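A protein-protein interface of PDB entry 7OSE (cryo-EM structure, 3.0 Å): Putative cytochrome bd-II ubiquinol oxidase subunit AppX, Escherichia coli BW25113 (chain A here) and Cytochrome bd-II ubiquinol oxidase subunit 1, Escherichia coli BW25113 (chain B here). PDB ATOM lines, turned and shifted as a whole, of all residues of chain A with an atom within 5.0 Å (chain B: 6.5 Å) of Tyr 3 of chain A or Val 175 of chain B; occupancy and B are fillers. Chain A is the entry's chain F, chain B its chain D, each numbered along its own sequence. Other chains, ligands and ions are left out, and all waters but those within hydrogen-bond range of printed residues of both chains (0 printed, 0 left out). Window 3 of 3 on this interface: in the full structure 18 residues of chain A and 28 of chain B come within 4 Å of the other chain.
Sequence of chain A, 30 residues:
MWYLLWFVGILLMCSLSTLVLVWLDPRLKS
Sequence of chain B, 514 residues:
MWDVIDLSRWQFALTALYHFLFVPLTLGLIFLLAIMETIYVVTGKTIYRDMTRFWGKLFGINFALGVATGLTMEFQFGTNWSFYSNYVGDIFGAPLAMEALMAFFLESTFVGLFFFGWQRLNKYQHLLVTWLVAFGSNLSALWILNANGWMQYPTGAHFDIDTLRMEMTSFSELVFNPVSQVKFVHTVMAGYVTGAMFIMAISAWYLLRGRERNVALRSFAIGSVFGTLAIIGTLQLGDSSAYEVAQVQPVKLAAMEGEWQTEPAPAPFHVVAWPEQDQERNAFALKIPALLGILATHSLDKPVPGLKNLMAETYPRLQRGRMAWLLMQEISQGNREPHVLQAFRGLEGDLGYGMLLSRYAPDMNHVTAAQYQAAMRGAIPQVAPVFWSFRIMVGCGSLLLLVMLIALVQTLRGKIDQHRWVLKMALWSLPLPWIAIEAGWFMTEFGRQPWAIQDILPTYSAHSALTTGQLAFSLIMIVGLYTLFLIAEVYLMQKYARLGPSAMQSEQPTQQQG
Of the 17 printed residues of chain B, 6 touch a printed residue of chain A. Of the 7 printed residues of chain A, 4 touch a printed residue of chain B. Among the printed residues, 10 pairs touch across the chains.
OG of Ser 180 of chain B lies within hydrogen-bond range of OD1 of Asn 146 of chain B (3.1 Å). O of Val 175 of chain B sits close to OD1 of Asn 177 of chain B, at 3.1 Å.
Printed residues of chain B within 4 Å of Tyr 3 of chain A: Leu 142, Val 175, Ser 180, Gln 181 and Phe 184. Printed residues of chain A within 4 Å of Val 185 of chain B: Trp 2 (3.6 Å) and Trp 6 (3.9 Å). Printed residues of chain A within 4 Å of Ser 180 of chain B: Tyr 3 (2.9 Å). Printed residues of chain A within 4 Å of Gln 181 of chain B: Met 1 (2.9 Å), Trp 2 (3.4 Å) and Tyr 3 (3.5 Å). Of the printed residues of chain B, Met 1 of chain A touches Gln 181 (2.9 Å). The nearest printed residue of chain A that does not touch Val 175 of chain B is Met 1 of chain A (7.8 Å).
The side-chain hydroxyl of Tyr 3 of chain A sits at hydrogen-bond distance from the backbone carbonyl oxygen of Val 175 of chain B (2.9 Å). The backbone NH (N) of Trp 2 of chain A lies within hydrogen-bond range of the side-chain amide oxygen (OE1) of Gln 181 of chain B, at 3.4 Å. OE1 of Gln 181 of chain B lies within hydrogen-bond range of N of Met 1 of chain A, 2.9 Å away. The side-chain hydroxyl (OH) of Tyr 3 of chain A is in hydrogen-bond range of the side-chain hydroxyl (OG) of Ser 180 of chain B, at 2.9 Å.
Among the printed residues, pairs that only touch across the chains: Trp 2 of chain A with Val 185 of chain B (3.6 Å), Tyr 3 of chain A with Leu 142 of chain B (3.4 Å), Tyr 3 of chain A with Gln 181 of chain B (3.5 Å), Tyr 3 of chain A with Phe 184 of chain B (3.6 Å), Trp 6 of chain A with Phe 184 of chain B (3.3 Å) and Trp 6 of chain A with Val 185 of chain B (3.9 Å).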
ATOM      1  N   MET A   1     -18.374  26.570 -24.938  1.00  0.00           N
ATOM      2  CA  MET A   1     -18.793  25.507 -24.033  1.00  0.00           C
ATOM      3  C   MET A   1     -18.945  24.195 -24.794  1.00  0.00           C
ATOM      4  O   MET A   1     -19.316  23.171 -24.223  1.00  0.00           O
ATOM      5  CB  MET A   1     -20.105  25.881 -23.340  1.00  0.00           C
ATOM      6  CG  MET A   1     -20.349  25.162 -22.024  1.00  0.00           C
ATOM      7  SD  MET A   1     -21.838  25.732 -21.186  1.00  0.00           S
ATOM      8  CE  MET A   1     -23.088  25.297 -22.392  1.00  0.00           C
ATOM      9  N   TRP A   2     -18.645  24.232 -26.094  1.00  0.00           N
ATOM     10  CA  TRP A   2     -18.755  23.033 -26.918  1.00  0.00           C
ATOM     11  C   TRP A   2     -17.716  21.978 -26.565  1.00  0.00           C
ATOM     12  O   TRP A   2     -17.881  20.820 -26.952  1.00  0.00           O
ATOM     13  CB  TRP A   2     -18.628  23.389 -28.397  1.00  0.00           C
ATOM     14  CG  TRP A   2     -19.901  23.848 -29.025  1.00  0.00           C
ATOM     15  CD1 TRP A   2     -20.275  25.135 -29.273  1.00  0.00           C
ATOM     16  CD2 TRP A   2     -20.970  23.021 -29.494  1.00  0.00           C
ATOM     17  NE1 TRP A   2     -21.513  25.161 -29.865  1.00  0.00           N
ATOM     18  CE2 TRP A   2     -21.962  23.875 -30.012  1.00  0.00           C
ATOM     19  CE3 TRP A   2     -21.185  21.642 -29.523  1.00  0.00           C
ATOM     20  CZ2 TRP A   2     -23.149  23.395 -30.553  1.00  0.00           C
ATOM     21  CZ3 TRP A   2     -22.366  21.167 -30.061  1.00  0.00           C
ATOM     22  CH2 TRP A   2     -23.332  22.040 -30.568  1.00  0.00           C
ATOM     23  N   TYR A   3     -16.648  22.346 -25.856  1.00  0.00           N
ATOM     24  CA  TYR A   3     -15.635  21.358 -25.493  1.00  0.00           C
ATOM     25  C   TYR A   3     -16.182  20.361 -24.479  1.00  0.00           C
ATOM     26  O   TYR A   3     -16.048  19.143 -24.651  1.00  0.00           O
ATOM     27  CB  TYR A   3     -14.392  22.059 -24.945  1.00  0.00           C
ATOM     28  CG  TYR A   3     -13.772  23.056 -25.899  1.00  0.00           C
ATOM     29  CD1 TYR A   3     -13.943  22.939 -27.270  1.00  0.00           C
ATOM     30  CD2 TYR A   3     -13.013  24.116 -25.424  1.00  0.00           C
ATOM     31  CE1 TYR A   3     -13.381  23.849 -28.139  1.00  0.00           C
ATOM     32  CE2 TYR A   3     -12.444  25.030 -26.287  1.00  0.00           C
ATOM     33  CZ  TYR A   3     -12.631  24.891 -27.643  1.00  0.00           C
ATOM     34  OH  TYR A   3     -12.067  25.798 -28.508  1.00  0.00           O
ATOM     35  N   LEU A   4     -16.815  20.864 -23.416  1.00  0.00           N
ATOM     36  CA  LEU A   4     -17.429  19.979 -22.433  1.00  0.00           C
ATOM     37  C   LEU A   4     -18.566  19.184 -23.056  1.00  0.00           C
ATOM     38  O   LEU A   4     -18.756  18.000 -22.744  1.00  0.00           O
ATOM     39  CB  LEU A   4     -17.930  20.791 -21.240  1.00  0.00           C
ATOM     40  CG  LEU A   4     -18.465  19.985 -20.058  1.00  0.00           C
ATOM     41  CD1 LEU A   4     -17.404  19.027 -19.549  1.00  0.00           C
ATOM     42  CD2 LEU A   4     -18.926  20.912 -18.949  1.00  0.00           C
ATOM     43  N   LEU A   5     -19.339  19.822 -23.937  1.00  0.00           N
ATOM     44  CA  LEU A   5     -20.408  19.114 -24.629  1.00  0.00           C
ATOM     45  C   LEU A   5     -19.850  17.971 -25.463  1.00  0.00           C
ATOM     46  O   LEU A   5     -20.404  16.869 -25.462  1.00  0.00           O
ATOM     47  CB  LEU A   5     -21.200  20.089 -25.503  1.00  0.00           C
ATOM     48  CG  LEU A   5     -22.648  19.739 -25.853  1.00  0.00           C
ATOM     49  CD1 LEU A   5     -23.405  20.995 -26.246  1.00  0.00           C
ATOM     50  CD2 LEU A   5     -22.725  18.708 -26.967  1.00  0.00           C
ATOM     51  N   TRP A   6     -18.744  18.208 -26.172  1.00  0.00           N
ATOM     52  CA  TRP A   6     -18.125  17.146 -26.955  1.00  0.00           C
ATOM     53  C   TRP A   6     -17.610  16.029 -26.062  1.00  0.00           C
ATOM     54  O   TRP A   6     -17.731  14.850 -26.406  1.00  0.00           O
ATOM     55  CB  TRP A   6     -16.981  17.699 -27.802  1.00  0.00           C
ATOM     56  CG  TRP A   6     -16.025  16.623 -28.218  1.00  0.00           C
ATOM     57  CD1 TRP A   6     -16.140  15.800 -29.297  1.00  0.00           C
ATOM     58  CD2 TRP A   6     -14.820  16.238 -27.545  1.00  0.00           C
ATOM     59  NE1 TRP A   6     -15.078  14.932 -29.345  1.00  0.00           N
ATOM     60  CE2 TRP A   6     -14.254  15.179 -28.279  1.00  0.00           C
ATOM     61  CE3 TRP A   6     -14.165  16.686 -26.395  1.00  0.00           C
ATOM     62  CZ2 TRP A   6     -13.064  14.565 -27.903  1.00  0.00           C
ATOM     63  CZ3 TRP A   6     -12.984  16.074 -26.024  1.00  0.00           C
ATOM     64  CH2 TRP A   6     -12.446  15.026 -26.776  1.00  0.00           C
ATOM     65  N   PHE A   7     -17.004  16.380 -24.929  1.00  0.00           N
ATOM     66  CA  PHE A   7     -16.490  15.363 -24.015  1.00  0.00           C
ATOM     67  C   PHE A   7     -17.614  14.462 -23.518  1.00  0.00           C
ATOM     68  O   PHE A   7     -17.533  13.224 -23.599  1.00  0.00           O
ATOM     69  CB  PHE A   7     -15.776  16.047 -22.849  1.00  0.00           C
ATOM     70  CG  PHE A   7     -15.089  15.102 -21.913  1.00  0.00           C
ATOM     71  CD1 PHE A   7     -13.852  14.568 -22.230  1.00  0.00           C
ATOM     72  CD2 PHE A   7     -15.665  14.765 -20.702  1.00  0.00           C
ATOM     73  CE1 PHE A   7     -13.213  13.705 -21.365  1.00  0.00           C
ATOM     74  CE2 PHE A   7     -15.029  13.903 -19.833  1.00  0.00           C
ATOM     75  CZ  PHE A   7     -13.802  13.372 -20.165  1.00  0.00           C
ATOM     76  N   MET B  98       1.072  24.137 -26.894  1.00  0.00           N
ATOM     77  CA  MET B  98       0.329  23.404 -25.874  1.00  0.00           C
ATOM     78  C   MET B  98      -0.100  22.028 -26.363  1.00  0.00           C
ATOM     79  O   MET B  98      -0.101  21.064 -25.583  1.00  0.00           O
ATOM     80  CB  MET B  98      -0.889  24.213 -25.433  1.00  0.00           C
ATOM     81  CG  MET B  98      -1.477  23.764 -24.112  1.00  0.00           C
ATOM     82  SD  MET B  98      -2.766  24.872 -23.522  1.00  0.00           S
ATOM     83  CE  MET B  98      -1.960  26.458 -23.718  1.00  0.00           C
ATOM     84  N   LEU B 142      -8.162  19.104 -31.066  1.00  0.00           N
ATOM     85  CA  LEU B 142      -8.780  20.250 -30.410  1.00  0.00           C
ATOM     86  C   LEU B 142      -7.900  21.487 -30.517  1.00  0.00           C
ATOM     87  O   LEU B 142      -8.356  22.552 -30.945  1.00  0.00           O
ATOM     88  CB  LEU B 142      -9.065  19.925 -28.944  1.00  0.00           C
ATOM     89  CG  LEU B 142      -9.389  21.134 -28.068  1.00  0.00           C
ATOM     90  CD1 LEU B 142     -10.685  21.770 -28.522  1.00  0.00           C
ATOM     91  CD2 LEU B 142      -9.467  20.745 -26.602  1.00  0.00           C
ATOM     92  N   TRP B 143      -6.629  21.361 -30.144  1.00  0.00           N
ATOM     93  CA  TRP B 143      -5.752  22.530 -30.152  1.00  0.00           C
ATOM     94  C   TRP B 143      -5.450  23.001 -31.572  1.00  0.00           C
ATOM     95  O   TRP B 143      -5.433  24.213 -31.842  1.00  0.00           O
ATOM     96  CB  TRP B 143      -4.465  22.228 -29.391  1.00  0.00           C
ATOM     97  CG  TRP B 143      -4.687  22.075 -27.922  1.00  0.00           C
ATOM     98  CD1 TRP B 143      -4.498  20.950 -27.176  1.00  0.00           C
ATOM     99  CD2 TRP B 143      -5.159  23.080 -27.018  1.00  0.00           C
ATOM    100  NE1 TRP B 143      -4.815  21.194 -25.863  1.00  0.00           N
ATOM    101  CE2 TRP B 143      -5.223  22.495 -25.740  1.00  0.00           C
ATOM    102  CE3 TRP B 143      -5.528  24.420 -27.166  1.00  0.00           C
ATOM    103  CZ2 TRP B 143      -5.644  23.201 -24.617  1.00  0.00           C
ATOM    104  CZ3 TRP B 143      -5.945  25.120 -26.050  1.00  0.00           C
ATOM    105  CH2 TRP B 143      -6.000  24.510 -24.792  1.00  0.00           C
ATOM    106  N   ASN B 146      -8.405  24.761 -32.795  1.00  0.00           N
ATOM    107  CA  ASN B 146      -8.502  26.055 -32.129  1.00  0.00           C
ATOM    108  C   ASN B 146      -7.629  27.090 -32.824  1.00  0.00           C
ATOM    109  O   ASN B 146      -8.052  28.232 -33.042  1.00  0.00           O
ATOM    110  CB  ASN B 146      -8.109  25.919 -30.658  1.00  0.00           C
ATOM    111  CG  ASN B 146      -8.137  27.242 -29.924  1.00  0.00           C
ATOM    112  OD1 ASN B 146      -8.929  28.126 -30.244  1.00  0.00           O
ATOM    113  ND2 ASN B 146      -7.266  27.387 -28.933  1.00  0.00           N
ATOM    114  N   SER B 170      -6.150  38.479 -24.906  1.00  0.00           N
ATOM    115  CA  SER B 170      -6.908  37.733 -23.906  1.00  0.00           C
ATOM    116  C   SER B 170      -6.897  36.262 -24.297  1.00  0.00           C
ATOM    117  O   SER B 170      -7.442  35.891 -25.341  1.00  0.00           O
ATOM    118  CB  SER B 170      -8.334  38.260 -23.789  1.00  0.00           C
ATOM    119  OG  SER B 170      -9.111  37.439 -22.937  1.00  0.00           O
ATOM    120  N   PHE B 171      -6.279  35.432 -23.456  1.00  0.00           N
ATOM    121  CA  PHE B 171      -6.218  33.999 -23.721  1.00  0.00           C
ATOM    122  C   PHE B 171      -7.589  33.345 -23.603  1.00  0.00           C
ATOM    123  O   PHE B 171      -7.880  32.384 -24.326  1.00  0.00           O
ATOM    124  CB  PHE B 171      -5.229  33.346 -22.759  1.00  0.00           C
ATOM    125  CG  PHE B 171      -4.908  31.918 -23.083  1.00  0.00           C
ATOM    126  CD1 PHE B 171      -4.178  31.598 -24.213  1.00  0.00           C
ATOM    127  CD2 PHE B 171      -5.317  30.896 -22.244  1.00  0.00           C
ATOM    128  CE1 PHE B 171      -3.875  30.284 -24.510  1.00  0.00           C
ATOM    129  CE2 PHE B 171      -5.014  29.581 -22.533  1.00  0.00           C
ATOM    130  CZ  PHE B 171      -4.292  29.275 -23.669  1.00  0.00           C
ATOM    131  N   SER B 172      -8.435  33.848 -22.701  1.00  0.00           N
ATOM    132  CA  SER B 172      -9.735  33.227 -22.468  1.00  0.00           C
ATOM    133  C   SER B 172     -10.595  33.254 -23.724  1.00  0.00           C
ATOM    134  O   SER B 172     -11.191  32.240 -24.104  1.00  0.00           O
ATOM    135  CB  SER B 172     -10.447  33.928 -21.311  1.00  0.00           C
ATOM    136  OG  SER B 172     -11.730  33.371 -21.090  1.00  0.00           O
ATOM    137  N   GLU B 173     -10.671  34.407 -24.390  1.00  0.00           N
ATOM    138  CA  GLU B 173     -11.446  34.487 -25.620  1.00  0.00           C
ATOM    139  C   GLU B 173     -10.705  33.900 -26.812  1.00  0.00           C
ATOM    140  O   GLU B 173     -11.339  33.580 -27.823  1.00  0.00           O
ATOM    141  CB  GLU B 173     -11.841  35.935 -25.910  1.00  0.00           C
ATOM    142  CG  GLU B 173     -10.676  36.884 -26.075  1.00  0.00           C
ATOM    143  CD  GLU B 173     -11.100  38.335 -25.967  1.00  0.00           C
ATOM    144  OE1 GLU B 173     -12.274  38.585 -25.623  1.00  0.00           O
ATOM    145  OE2 GLU B 173     -10.263  39.224 -26.224  1.00  0.00           O
ATOM    146  N   LEU B 174      -9.382  33.759 -26.719  1.00  0.00           N
ATOM    147  CA  LEU B 174      -8.647  33.034 -27.749  1.00  0.00           C
ATOM    148  C   LEU B 174      -9.018  31.557 -27.749  1.00  0.00           C
ATOM    149  O   LEU B 174      -9.222  30.963 -28.813  1.00  0.00           O
ATOM    150  CB  LEU B 174      -7.144  33.208 -27.541  1.00  0.00           C
ATOM    151  CG  LEU B 174      -6.232  32.128 -28.129  1.00  0.00           C
ATOM    152  CD1 LEU B 174      -6.268  32.144 -29.644  1.00  0.00           C
ATOM    153  CD2 LEU B 174      -4.813  32.304 -27.629  1.00  0.00           C
ATOM    154  N   VAL B 175      -9.104  30.949 -26.565  1.00  0.00           N
ATOM    155  CA  VAL B 175      -9.450  29.534 -26.487  1.00  0.00           C
ATOM    156  C   VAL B 175     -10.915  29.312 -26.844  1.00  0.00           C
ATOM    157  O   VAL B 175     -11.251  28.391 -27.597  1.00  0.00           O
ATOM    158  CB  VAL B 175      -9.122  28.979 -25.091  1.00  0.00           C
ATOM    159  CG1 VAL B 175      -9.504  27.513 -25.006  1.00  0.00           C
ATOM    160  CG2 VAL B 175      -7.652  29.163 -24.788  1.00  0.00           C
ATOM    161  N   PHE B 176     -11.809  30.148 -26.315  1.00  0.00           N
ATOM    162  CA  PHE B 176     -13.245  29.922 -26.410  1.00  0.00           C
ATOM    163  C   PHE B 176     -13.906  30.762 -27.497  1.00  0.00           C
ATOM    164  O   PHE B 176     -15.052  31.192 -27.331  1.00  0.00           O
ATOM    165  CB  PHE B 176     -13.911  30.191 -25.062  1.00  0.00           C
ATOM    166  CG  PHE B 176     -13.461  29.268 -23.966  1.00  0.00           C
ATOM    167  CD1 PHE B 176     -13.976  27.989 -23.866  1.00  0.00           C
ATOM    168  CD2 PHE B 176     -12.530  29.685 -23.032  1.00  0.00           C
ATOM    169  CE1 PHE B 176     -13.566  27.140 -22.858  1.00  0.00           C
ATOM    170  CE2 PHE B 176     -12.115  28.840 -22.022  1.00  0.00           C
ATOM    171  CZ  PHE B 176     -12.636  27.566 -21.935  1.00  0.00           C
ATOM    172  N   ASN B 177     -13.214  31.009 -28.603  1.00  0.00           N
ATOM    173  CA  ASN B 177     -13.837  31.731 -29.703  1.00  0.00           C
ATOM    174  C   ASN B 177     -14.944  30.879 -30.319  1.00  0.00           C
ATOM    175  O   ASN B 177     -14.824  29.652 -30.377  1.00  0.00           O
ATOM    176  CB  ASN B 177     -12.802  32.105 -30.761  1.00  0.00           C
ATOM    177  CG  ASN B 177     -11.816  30.995 -31.023  1.00  0.00           C
ATOM    178  OD1 ASN B 177     -11.542  30.178 -30.146  1.00  0.00           O
ATOM    179  ND2 ASN B 177     -11.271  30.959 -32.233  1.00  0.00           N
ATOM    180  N   SER B 180     -13.940  28.309 -33.258  1.00  0.00           N
ATOM    181  CA  SER B 180     -13.022  27.211 -32.970  1.00  0.00           C
ATOM    182  C   SER B 180     -13.739  26.019 -32.349  1.00  0.00           C
ATOM    183  O   SER B 180     -13.468  24.871 -32.712  1.00  0.00           O
ATOM    184  CB  SER B 180     -11.905  27.693 -32.052  1.00  0.00           C
ATOM    185  OG  SER B 180     -11.455  26.645 -31.214  1.00  0.00           O
ATOM    186  N   GLN B 181     -14.643  26.269 -31.400  1.00  0.00           N
ATOM    187  CA  GLN B 181     -15.334  25.169 -30.731  1.00  0.00           C
ATOM    188  C   GLN B 181     -16.167  24.365 -31.720  1.00  0.00           C
ATOM    189  O   GLN B 181     -16.103  23.128 -31.751  1.00  0.00           O
ATOM    190  CB  GLN B 181     -16.217  25.714 -29.610  1.00  0.00           C
ATOM    191  CG  GLN B 181     -15.515  26.649 -28.647  1.00  0.00           C
ATOM    192  CD  GLN B 181     -16.456  27.205 -27.600  1.00  0.00           C
ATOM    193  OE1 GLN B 181     -17.675  27.091 -27.725  1.00  0.00           O
ATOM    194  NE2 GLN B 181     -15.897  27.807 -26.558  1.00  0.00           N
ATOM    195  N   VAL B 182     -16.961  25.060 -32.535  1.00  0.00           N
ATOM    196  CA  VAL B 182     -17.809  24.383 -33.507  1.00  0.00           C
ATOM    197  C   VAL B 182     -16.957  23.636 -34.522  1.00  0.00           C
ATOM    198  O   VAL B 182     -17.260  22.492 -34.882  1.00  0.00           O
ATOM    199  CB  VAL B 182     -18.752  25.392 -34.184  1.00  0.00           C
ATOM    200  CG1 VAL B 182     -19.787  24.666 -35.012  1.00  0.00           C
ATOM    201  CG2 VAL B 182     -19.425  26.263 -33.141  1.00  0.00           C
ATOM    202  N   PHE B 184     -13.935  22.404 -34.109  1.00  0.00           N
ATOM    203  CA  PHE B 184     -13.336  21.243 -33.462  1.00  0.00           C
ATOM    204  C   PHE B 184     -14.335  20.105 -33.339  1.00  0.00           C
ATOM    205  O   PHE B 184     -14.048  18.965 -33.731  1.00  0.00           O
ATOM    206  CB  PHE B 184     -12.791  21.640 -32.090  1.00  0.00           C
ATOM    207  CG  PHE B 184     -12.869  20.547 -31.063  1.00  0.00           C
ATOM    208  CD1 PHE B 184     -12.014  19.463 -31.116  1.00  0.00           C
ATOM    209  CD2 PHE B 184     -13.792  20.613 -30.035  1.00  0.00           C
ATOM    210  CE1 PHE B 184     -12.082  18.464 -30.168  1.00  0.00           C
ATOM    211  CE2 PHE B 184     -13.865  19.615 -29.087  1.00  0.00           C
ATOM    212  CZ  PHE B 184     -13.009  18.540 -29.154  1.00  0.00           C
ATOM    213  N   VAL B 185     -15.521  20.391 -32.795  1.00  0.00           N
ATOM    214  CA  VAL B 185     -16.503  19.326 -32.610  1.00  0.00           C
ATOM    215  C   VAL B 185     -16.907  18.742 -33.957  1.00  0.00           C
ATOM    216  O   VAL B 185     -17.041  17.520 -34.106  1.00  0.00           O
ATOM    217  CB  VAL B 185     -17.723  19.835 -31.821  1.00  0.00           C
ATOM    218  CG1 VAL B 185     -18.659  18.684 -31.514  1.00  0.00           C
ATOM    219  CG2 VAL B 185     -17.282  20.493 -30.532  1.00  0.00           C
